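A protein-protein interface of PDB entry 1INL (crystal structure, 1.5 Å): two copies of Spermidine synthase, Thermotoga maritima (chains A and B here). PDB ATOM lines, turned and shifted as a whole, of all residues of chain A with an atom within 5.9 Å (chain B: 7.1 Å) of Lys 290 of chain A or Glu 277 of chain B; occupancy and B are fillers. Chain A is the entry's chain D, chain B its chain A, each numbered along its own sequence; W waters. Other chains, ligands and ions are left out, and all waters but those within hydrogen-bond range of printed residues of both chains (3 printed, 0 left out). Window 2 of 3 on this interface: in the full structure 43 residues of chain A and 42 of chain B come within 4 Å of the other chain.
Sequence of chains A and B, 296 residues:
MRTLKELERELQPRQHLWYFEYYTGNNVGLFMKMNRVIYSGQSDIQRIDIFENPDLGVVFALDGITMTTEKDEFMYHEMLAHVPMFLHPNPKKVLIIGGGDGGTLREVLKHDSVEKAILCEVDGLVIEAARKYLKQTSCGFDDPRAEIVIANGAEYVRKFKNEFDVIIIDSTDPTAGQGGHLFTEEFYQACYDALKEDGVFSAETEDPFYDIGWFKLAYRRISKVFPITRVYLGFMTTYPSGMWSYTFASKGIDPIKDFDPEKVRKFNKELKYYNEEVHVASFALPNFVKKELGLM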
ATOM      1  N   PHE A 283     -10.560 -13.363  17.356  1.00  0.00           N
ATOM      2  CA  PHE A 283     -11.687 -14.020  18.009  1.00  0.00           C
ATOM      3  C   PHE A 283     -11.835 -13.703  19.500  1.00  0.00           C
ATOM      4  O   PHE A 283     -12.812 -14.108  20.134  1.00  0.00           O
ATOM      5  CB  PHE A 283     -11.643 -15.533  17.761  1.00  0.00           C
ATOM      6  CG  PHE A 283     -12.028 -15.917  16.359  1.00  0.00           C
ATOM      7  CD1 PHE A 283     -11.068 -15.999  15.356  1.00  0.00           C
ATOM      8  CD2 PHE A 283     -13.361 -16.147  16.034  1.00  0.00           C
ATOM      9  CE1 PHE A 283     -11.429 -16.303  14.041  1.00  0.00           C
ATOM     10  CE2 PHE A 283     -13.734 -16.451  14.723  1.00  0.00           C
ATOM     11  CZ  PHE A 283     -12.765 -16.527  13.729  1.00  0.00           C
ATOM     12  N   ALA A 284     -10.869 -12.970  20.048  1.00  0.00           N
ATOM     13  CA  ALA A 284     -10.903 -12.569  21.454  1.00  0.00           C
ATOM     14  C   ALA A 284     -11.796 -11.334  21.540  1.00  0.00           C
ATOM     15  O   ALA A 284     -11.453 -10.275  21.009  1.00  0.00           O
ATOM     16  CB  ALA A 284      -9.500 -12.250  21.945  1.00  0.00           C
ATOM     17  N   LEU A 285     -12.938 -11.473  22.209  1.00  0.00           N
ATOM     18  CA  LEU A 285     -13.898 -10.377  22.320  1.00  0.00           C
ATOM     19  C   LEU A 285     -13.856  -9.626  23.645  1.00  0.00           C
ATOM     20  O   LEU A 285     -13.759 -10.237  24.708  1.00  0.00           O
ATOM     21  CB  LEU A 285     -15.321 -10.909  22.107  1.00  0.00           C
ATOM     22  CG  LEU A 285     -15.583 -11.800  20.892  1.00  0.00           C
ATOM     23  CD1 LEU A 285     -17.061 -12.158  20.840  1.00  0.00           C
ATOM     24  CD2 LEU A 285     -15.161 -11.078  19.619  1.00  0.00           C
ATOM     25  N   PRO A 286     -13.886  -8.284  23.594  1.00  0.00           N
ATOM     26  CA  PRO A 286     -13.865  -7.480  24.821  1.00  0.00           C
ATOM     27  C   PRO A 286     -15.143  -7.787  25.596  1.00  0.00           C
ATOM     28  O   PRO A 286     -16.140  -8.215  25.007  1.00  0.00           O
ATOM     29  CB  PRO A 286     -13.878  -6.049  24.287  1.00  0.00           C
ATOM     30  CG  PRO A 286     -13.147  -6.171  22.985  1.00  0.00           C
ATOM     31  CD  PRO A 286     -13.765  -7.423  22.406  1.00  0.00           C
ATOM     32  N   ASN A 287     -15.124  -7.553  26.905  1.00  0.00           N
ATOM     33  CA  ASN A 287     -16.285  -7.840  27.741  1.00  0.00           C
ATOM     34  C   ASN A 287     -17.607  -7.240  27.279  1.00  0.00           C
ATOM     35  O   ASN A 287     -18.626  -7.928  27.294  1.00  0.00           O
ATOM     36  CB  ASN A 287     -16.021  -7.455  29.200  1.00  0.00           C
ATOM     37  CG  ASN A 287     -15.109  -8.438  29.914  1.00  0.00           C
ATOM     38  OD1 ASN A 287     -14.745  -9.484  29.371  1.00  0.00           O
ATOM     39  ND2 ASN A 287     -14.739  -8.108  31.146  1.00  0.00           N
ATOM     40  N   PHE A 288     -17.602  -5.982  26.835  1.00  0.00           N
ATOM     41  CA  PHE A 288     -18.857  -5.366  26.406  1.00  0.00           C
ATOM     42  C   PHE A 288     -19.482  -6.056  25.199  1.00  0.00           C
ATOM     43  O   PHE A 288     -20.704  -6.116  25.086  1.00  0.00           O
ATOM     44  CB  PHE A 288     -18.720  -3.846  26.194  1.00  0.00           C
ATOM     45  CG  PHE A 288     -18.075  -3.447  24.891  1.00  0.00           C
ATOM     46  CD1 PHE A 288     -16.690  -3.402  24.766  1.00  0.00           C
ATOM     47  CD2 PHE A 288     -18.857  -3.058  23.805  1.00  0.00           C
ATOM     48  CE1 PHE A 288     -16.091  -2.972  23.578  1.00  0.00           C
ATOM     49  CE2 PHE A 288     -18.269  -2.626  22.613  1.00  0.00           C
ATOM     50  CZ  PHE A 288     -16.884  -2.583  22.502  1.00  0.00           C
ATOM     51  N   VAL A 289     -18.644  -6.610  24.327  1.00  0.00           N
ATOM     52  CA  VAL A 289     -19.126  -7.320  23.144  1.00  0.00           C
ATOM     53  C   VAL A 289     -19.711  -8.671  23.564  1.00  0.00           C
ATOM     54  O   VAL A 289     -20.783  -9.061  23.099  1.00  0.00           O
ATOM     55  CB  VAL A 289     -17.995  -7.520  22.106  1.00  0.00           C
ATOM     56  CG1 VAL A 289     -18.510  -8.287  20.897  1.00  0.00           C
ATOM     57  CG2 VAL A 289     -17.456  -6.165  21.661  1.00  0.00           C
ATOM     58  N   LYS A 290     -19.022  -9.360  24.469  1.00  0.00           N
ATOM     59  CA  LYS A 290     -19.490 -10.653  24.966  1.00  0.00           C
ATOM     60  C   LYS A 290     -20.843 -10.496  25.657  1.00  0.00           C
ATOM     61  O   LYS A 290     -21.735 -11.327  25.483  1.00  0.00           O
ATOM     62  CB  LYS A 290     -18.470 -11.254  25.940  1.00  0.00           C
ATOM     63  CG  LYS A 290     -17.127 -11.554  25.300  1.00  0.00           C
ATOM     64  CD  LYS A 290     -16.036 -11.847  26.322  1.00  0.00           C
ATOM     65  CE  LYS A 290     -16.184 -13.213  26.952  1.00  0.00           C
ATOM     66  NZ  LYS A 290     -15.020 -13.519  27.832  1.00  0.00           N
ATOM     67  N   LYS A 291     -21.002  -9.409  26.408  1.00  0.00           N
ATOM     68  CA  LYS A 291     -22.248  -9.133  27.120  1.00  0.00           C
ATOM     69  C   LYS A 291     -23.401  -8.885  26.144  1.00  0.00           C
ATOM     70  O   LYS A 291     -24.517  -9.357  26.362  1.00  0.00           O
ATOM     71  CB  LYS A 291     -22.071  -7.932  28.053  1.00  0.00           C
ATOM     72  CG  LYS A 291     -23.236  -7.694  29.001  1.00  0.00           C
ATOM     73  CD  LYS A 291     -22.938  -6.549  29.959  1.00  0.00           C
ATOM     74  CE  LYS A 291     -24.067  -6.350  30.962  1.00  0.00           C
ATOM     75  NZ  LYS A 291     -25.353  -5.985  30.307  1.00  0.00           N
ATOM     76  N   GLU A 292     -23.122  -8.166  25.058  1.00  0.00           N
ATOM     77  CA  GLU A 292     -24.139  -7.873  24.050  1.00  0.00           C
ATOM     78  C   GLU A 292     -24.584  -9.128  23.300  1.00  0.00           C
ATOM     79  O   GLU A 292     -25.705  -9.189  22.794  1.00  0.00           O
ATOM     80  CB  GLU A 292     -23.629  -6.831  23.049  1.00  0.00           C
ATOM     81  CG  GLU A 292     -23.448  -5.427  23.625  1.00  0.00           C
ATOM     82  CD  GLU A 292     -24.756  -4.759  24.041  1.00  0.00           C
ATOM     83  OE1 GLU A 292     -25.840  -5.194  23.595  1.00  0.00           O
ATOM     84  OE2 GLU A 292     -24.694  -3.781  24.815  1.00  0.00           O
ATOM     85  N   LEU A 293     -23.698 -10.120  23.225  1.00  0.00           N
ATOM     86  CA  LEU A 293     -23.996 -11.373  22.536  1.00  0.00           C
ATOM     87  C   LEU A 293     -24.519 -12.457  23.476  1.00  0.00           C
ATOM     88  O   LEU A 293     -24.797 -13.578  23.044  1.00  0.00           O
ATOM     89  CB  LEU A 293     -22.755 -11.886  21.803  1.00  0.00           C
ATOM     90  CG  LEU A 293     -22.195 -10.994  20.694  1.00  0.00           C
ATOM     91  CD1 LEU A 293     -20.922 -11.602  20.137  1.00  0.00           C
ATOM     92  CD2 LEU A 293     -23.234 -10.816  19.598  1.00  0.00           C
ATOM     93  N   GLY A 294     -24.645 -12.118  24.756  1.00  0.00           N
ATOM     94  CA  GLY A 294     -25.134 -13.073  25.736  1.00  0.00           C
ATOM     95  C   GLY A 294     -24.106 -14.116  26.125  1.00  0.00           C
ATOM     96  O   GLY A 294     -24.439 -15.124  26.749  1.00  0.00           O
ATOM     97  N   LEU A 295     -22.855 -13.881  25.740  1.00  0.00           N
ATOM     98  CA  LEU A 295     -21.760 -14.791  26.054  1.00  0.00           C
ATOM     99  C   LEU A 295     -21.167 -14.444  27.420  1.00  0.00           C
ATOM    100  O   LEU A 295     -20.173 -15.034  27.845  1.00  0.00           O
ATOM    101  CB  LEU A 295     -20.679 -14.707  24.972  1.00  0.00           C
ATOM    102  CG  LEU A 295     -21.123 -15.017  23.538  1.00  0.00           C
ATOM    103  CD1 LEU A 295     -19.975 -14.778  22.574  1.00  0.00           C
ATOM    104  CD2 LEU A 295     -21.618 -16.454  23.437  1.00  0.00           C
ATOM    105  N   MET A 296     -21.803 -13.494  28.102  1.00  0.00           N
ATOM    106  CA  MET A 296     -21.368 -13.040  29.419  1.00  0.00           C
ATOM    107  C   MET A 296     -22.505 -12.298  30.116  1.00  0.00           C
ATOM    108  O   MET A 296     -22.839 -12.587  31.266  1.00  0.00           O
ATOM    109  CB  MET A 296     -20.154 -12.117  29.277  1.00  0.00           C
ATOM    110  CG  MET A 296     -19.633 -11.548  30.582  1.00  0.00           C
ATOM    111  SD  MET A 296     -18.170 -10.532  30.327  1.00  0.00           S
ATOM    112  CE  MET A 296     -16.875 -11.703  30.732  1.00  0.00           C
ATOM    113  N   PHE B 259       2.467 -13.555  31.962  1.00  0.00           N
ATOM    114  CA  PHE B 259       1.078 -13.192  32.226  1.00  0.00           C
ATOM    115  C   PHE B 259       0.354 -14.338  32.935  1.00  0.00           C
ATOM    116  O   PHE B 259       0.415 -15.486  32.490  1.00  0.00           O
ATOM    117  CB  PHE B 259       0.360 -12.862  30.910  1.00  0.00           C
ATOM    118  CG  PHE B 259      -1.092 -12.506  31.078  1.00  0.00           C
ATOM    119  CD1 PHE B 259      -1.480 -11.473  31.928  1.00  0.00           C
ATOM    120  CD2 PHE B 259      -2.077 -13.208  30.385  1.00  0.00           C
ATOM    121  CE1 PHE B 259      -2.823 -11.144  32.086  1.00  0.00           C
ATOM    122  CE2 PHE B 259      -3.426 -12.885  30.536  1.00  0.00           C
ATOM    123  CZ  PHE B 259      -3.798 -11.851  31.388  1.00  0.00           C
ATOM    124  N   PRO B 261      -3.241 -15.346  33.752  1.00  0.00           N
ATOM    125  CA  PRO B 261      -4.659 -15.086  33.495  1.00  0.00           C
ATOM    126  C   PRO B 261      -5.568 -15.202  34.711  1.00  0.00           C
ATOM    127  O   PRO B 261      -6.621 -14.570  34.751  1.00  0.00           O
ATOM    128  CB  PRO B 261      -5.007 -16.111  32.412  1.00  0.00           C
ATOM    129  CG  PRO B 261      -4.024 -17.217  32.648  1.00  0.00           C
ATOM    130  CD  PRO B 261      -2.756 -16.458  32.917  1.00  0.00           C
ATOM    131  N   VAL B 264      -6.626 -11.946  36.402  1.00  0.00           N
ATOM    132  CA  VAL B 264      -7.697 -11.256  35.699  1.00  0.00           C
ATOM    133  C   VAL B 264      -9.037 -11.953  35.918  1.00  0.00           C
ATOM    134  O   VAL B 264     -10.048 -11.301  36.166  1.00  0.00           O
ATOM    135  CB  VAL B 264      -7.395 -11.169  34.191  1.00  0.00           C
ATOM    136  CG1 VAL B 264      -8.470 -10.355  33.484  1.00  0.00           C
ATOM    137  CG2 VAL B 264      -6.013 -10.564  33.972  1.00  0.00           C
ATOM    138  N   TYR B 273     -14.028  -3.919  29.197  1.00  0.00           N
ATOM    139  CA  TYR B 273     -13.328  -4.236  27.954  1.00  0.00           C
ATOM    140  C   TYR B 273     -12.293  -5.336  28.170  1.00  0.00           C
ATOM    141  O   TYR B 273     -12.387  -6.427  27.603  1.00  0.00           O
ATOM    142  CB  TYR B 273     -12.626  -2.977  27.413  1.00  0.00           C
ATOM    143  CG  TYR B 273     -11.940  -3.142  26.069  1.00  0.00           C
ATOM    144  CD1 TYR B 273     -10.682  -3.738  25.966  1.00  0.00           C
ATOM    145  CD2 TYR B 273     -12.541  -2.678  24.898  1.00  0.00           C
ATOM    146  CE1 TYR B 273     -10.040  -3.870  24.732  1.00  0.00           C
ATOM    147  CE2 TYR B 273     -11.907  -2.803  23.663  1.00  0.00           C
ATOM    148  CZ  TYR B 273     -10.659  -3.400  23.586  1.00  0.00           C
ATOM    149  OH  TYR B 273     -10.035  -3.533  22.366  1.00  0.00           O
ATOM    150  N   TYR B 274     -11.321  -5.035  29.019  1.00  0.00           N
ATOM    151  CA  TYR B 274     -10.217  -5.934  29.315  1.00  0.00           C
ATOM    152  C   TYR B 274     -10.581  -7.267  29.973  1.00  0.00           C
ATOM    153  O   TYR B 274     -11.426  -7.326  30.861  1.00  0.00           O
ATOM    154  CB  TYR B 274      -9.197  -5.178  30.175  1.00  0.00           C
ATOM    155  CG  TYR B 274      -7.960  -5.956  30.550  1.00  0.00           C
ATOM    156  CD1 TYR B 274      -6.829  -5.941  29.737  1.00  0.00           C
ATOM    157  CD2 TYR B 274      -7.909  -6.687  31.737  1.00  0.00           C
ATOM    158  CE1 TYR B 274      -5.675  -6.633  30.099  1.00  0.00           C
ATOM    159  CE2 TYR B 274      -6.766  -7.378  32.103  1.00  0.00           C
ATOM    160  CZ  TYR B 274      -5.656  -7.347  31.286  1.00  0.00           C
ATOM    161  OH  TYR B 274      -4.524  -8.020  31.671  1.00  0.00           O
ATOM    162  N   ASN B 275      -9.951  -8.332  29.479  1.00  0.00           N
ATOM    163  CA  ASN B 275     -10.100  -9.688  30.010  1.00  0.00           C
ATOM    164  C   ASN B 275      -8.848 -10.473  29.609  1.00  0.00           C
ATOM    165  O   ASN B 275      -8.014  -9.967  28.854  1.00  0.00           O
ATOM    166  CB  ASN B 275     -11.398 -10.370  29.536  1.00  0.00           C
ATOM    167  CG  ASN B 275     -11.495 -10.502  28.029  1.00  0.00           C
ATOM    168  OD1 ASN B 275     -10.557 -10.938  27.366  1.00  0.00           O
ATOM    169  ND2 ASN B 275     -12.661 -10.174  27.488  1.00  0.00           N
ATOM    170  N   GLU B 276      -8.705 -11.699  30.105  1.00  0.00           N
ATOM    171  CA  GLU B 276      -7.519 -12.499  29.802  1.00  0.00           C
ATOM    172  C   GLU B 276      -7.263 -12.795  28.320  1.00  0.00           C
ATOM    173  O   GLU B 276      -6.109 -12.821  27.885  1.00  0.00           O
ATOM    174  CB  GLU B 276      -7.519 -13.801  30.615  1.00  0.00           C
ATOM    175  CG  GLU B 276      -8.619 -14.793  30.254  1.00  0.00           C
ATOM    176  CD  GLU B 276      -9.910 -14.595  31.034  1.00  0.00           C
ATOM    177  OE1 GLU B 276     -10.198 -13.464  31.486  1.00  0.00           O
ATOM    178  OE2 GLU B 276     -10.647 -15.591  31.198  1.00  0.00           O
ATOM    179  N   GLU B 277      -8.330 -13.015  27.552  1.00  0.00           N
ATOM    180  CA  GLU B 277      -8.210 -13.306  26.123  1.00  0.00           C
ATOM    181  C   GLU B 277      -7.746 -12.064  25.367  1.00  0.00           C
ATOM    182  O   GLU B 277      -6.873 -12.137  24.504  1.00  0.00           O
ATOM    183  CB  GLU B 277      -9.557 -13.769  25.564  1.00  0.00           C
ATOM    184  CG  GLU B 277     -10.172 -14.937  26.314  1.00  0.00           C
ATOM    185  CD  GLU B 277     -11.638 -15.131  25.979  1.00  0.00           C
ATOM    186  OE1 GLU B 277     -12.440 -14.211  26.263  1.00  0.00           O
ATOM    187  OE2 GLU B 277     -11.987 -16.199  25.433  1.00  0.00           O
ATOM    188  N   VAL B 278      -8.326 -10.921  25.721  1.00  0.00           N
ATOM    189  CA  VAL B 278      -7.979  -9.649  25.098  1.00  0.00           C
ATOM    190  C   VAL B 278      -6.544  -9.234  25.420  1.00  0.00           C
ATOM    191  O   VAL B 278      -5.861  -8.656  24.573  1.00  0.00           O
ATOM    192  CB  VAL B 278      -8.975  -8.538  25.514  1.00  0.00           C
ATOM    193  CG1 VAL B 278      -8.450  -7.163  25.119  1.00  0.00           C
ATOM    194  CG2 VAL B 278     -10.328  -8.782  24.850  1.00  0.00           C
ATOM    195  N   HIS B 279      -6.074  -9.551  26.625  1.00  0.00           N
ATOM    196  CA  HIS B 279      -4.710  -9.201  27.013  1.00  0.00           C
ATOM    197  C   HIS B 279      -3.711  -9.803  26.029  1.00  0.00           C
ATOM    198  O   HIS B 279      -2.880  -9.094  25.462  1.00  0.00           O
ATOM    199  CB  HIS B 279      -4.396  -9.694  28.431  1.00  0.00           C
ATOM    200  CG  HIS B 279      -3.020  -9.336  28.902  1.00  0.00           C
ATOM    201  ND1 HIS B 279      -1.892 -10.015  28.497  1.00  0.00           N
ATOM    202  CD2 HIS B 279      -2.592  -8.361  29.739  1.00  0.00           C
ATOM    203  CE1 HIS B 279      -0.827  -9.472  29.061  1.00  0.00           C
ATOM    204  NE2 HIS B 279      -1.224  -8.467  29.820  1.00  0.00           N
ATOM    205  N   VAL B 280      -3.812 -11.111  25.814  1.00  0.00           N
ATOM    206  CA  VAL B 280      -2.913 -11.808  24.903  1.00  0.00           C
ATOM    207  C   VAL B 280      -3.132 -11.392  23.452  1.00  0.00           C
ATOM    208  O   VAL B 280      -2.174 -11.135  22.720  1.00  0.00           O
ATOM    209  CB  VAL B 280      -3.080 -13.343  25.032  1.00  0.00           C
ATOM    210  CG1 VAL B 280      -2.214 -14.065  24.005  1.00  0.00           C
ATOM    211  CG2 VAL B 280      -2.711 -13.789  26.439  1.00  0.00           C
ATOM    212  N   ALA B 281      -4.398 -11.290  23.057  1.00  0.00           N
ATOM    213  CA  ALA B 281      -4.764 -10.921  21.694  1.00  0.00           C
ATOM    214  C   ALA B 281      -4.286  -9.535  21.278  1.00  0.00           C
ATOM    215  O   ALA B 281      -3.908  -9.323  20.123  1.00  0.00           O
ATOM    216  CB  ALA B 281      -6.267 -11.019  21.516  1.00  0.00           C
ATOM    217  N   SER B 282      -4.276  -8.601  22.224  1.00  0.00           N
ATOM    218  CA  SER B 282      -3.863  -7.235  21.920  1.00  0.00           C
ATOM    219  C   SER B 282      -2.434  -7.115  21.401  1.00  0.00           C
ATOM    220  O   SER B 282      -2.104  -6.145  20.723  1.00  0.00           O
ATOM    221  CB  SER B 282      -4.071  -6.321  23.131  1.00  0.00           C
ATOM    222  OG  SER B 282      -3.151  -6.608  24.171  1.00  0.00           O
HETATM  223  O   HOH W   1     -13.740 -13.945  23.605  1.00  0.00           O
HETATM  224  O   HOH W   2     -12.598  -9.303  32.573  1.00  0.00           O
HETATM  225  O   HOH W   3     -12.768 -14.528  29.445  1.00  0.00           O
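Water W2 lies within hydrogen-bond range of the side-chain amide nitrogen of Asn 287 of chain A (2.8 Å) and the backbone carbonyl oxygen of Tyr 274 of chain B (2.9 Å).
Water W3 lies within hydrogen-bond range of the side-chain amino group of Lys 290 of chain A (2.9 Å), the side-chain carboxylate of Glu 276 of chain B (2.9 Å) and the side-chain carboxylate of Glu 277 of chain B (3.2 Å).
Water W1 lies within hydrogen-bond range of the backbone NH of Leu 285 of chain A (3.0 Å) and the side-chain carboxylate of Glu 277 of chain B (3.0 Å).
Printed residues of chain B that touch a printed residue of chain A: Tyr 273, Tyr 274, Asn 275, Glu 277, Val 278 and Ala 281.
Hydrophobic or aromatic side chains of chain B within 4 Å of the printed part of chain A: Tyr 273, Val 278 and Ala 281.
Of the 14 printed residues of chain A, 6 touch a printed residue of chain B.
Printed residues of chain A that touch a printed residue of chain B: Ala 284, Leu 285, Pro 286, Asn 287, Phe 288 and Lys 290.
Among the printed residues, 13 pairs touch across the chains.
The backbone NH (N) of Glu 277 of chain B is in hydrogen-bond range of the side-chain amide oxygen (OD1) of Asn 275 of chain B (3.1 Å).
O of Val 278 of chain B lies close to OG of Ser 282 of chain B (3.4 Å).
The backbone NH (N) of Leu 295 of chain A lies within hydrogen-bond range of the backbone carbonyl oxygen (O) of Lys 290 of chain A, at 2.8 Å.
The side-chain sulfur of Met 296 of chain A sits close to the side-chain amide oxygen of Asn 287 of chain A, at 3.7 Å.
O of Lys 290 of chain A sits at hydrogen-bond distance from N of Met 296 of chain A, 3.4 Å away.
OD1 of Asn 275 of chain B lies within hydrogen-bond range of N of Val 278 of chain B.
Among the printed residues, merely in contact across the chains: Pro 286 of chain A with Tyr 273 of chain B, Ala 284 of chain A with Ala 281 of chain B, Ala 284 of chain A with Glu 277 of chain B, Leu 285 of chain A with Val 278 of chain B, Pro 286 of chain A with Val 278 of chain B, Phe 288 of chain A with Tyr 273 of chain B, Pro 286 of chain A with Asn 275 of chain B and Lys 290 of chain A with Asn 275 of chain B.
Lys 290 of chain A touches just these residues of chain B: Asn 275 (3.9 Å) and Glu 277 (3.1 Å).
Of the printed residues of chain A, Tyr 273 of chain B touches Pro 286, Asn 287 and Phe 288.
Printed residues of chain A within 4 Å of Asn 275 of chain B: Leu 285 (3.0 Å), Pro 286 (3.9 Å), Asn 287 (2.9 Å) and Lys 290 (3.9 Å).
Of the printed residues of chain A, Val 278 of chain B touches Leu 285 (3.7 Å) and Pro 286 (3.8 Å).
No position is printed for both chains.
OD1 of Asn 287 of chain A sits at hydrogen-bond distance from ND2 of Asn 275 of chain B, at 2.9 Å.
O of Tyr 273 of chain B is in hydrogen-bond range of N of Asn 287 of chain A (3.0 Å).
OE1 of Glu 277 of chain B is in salt-bridge range of NZ of Lys 290 of chain A, at 3.1 Å.
The side-chain amide nitrogen of Asn 275 of chain B sits at hydrogen-bond distance from the backbone carbonyl oxygen of Leu 285 of chain A (3.0 Å).
The backbone carbonyl oxygen (O) of Tyr 274 of chain B is in hydrogen-bond range of the side-chain amide nitrogen (ND2) of Asn 287 of chain A (3.4 Å).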
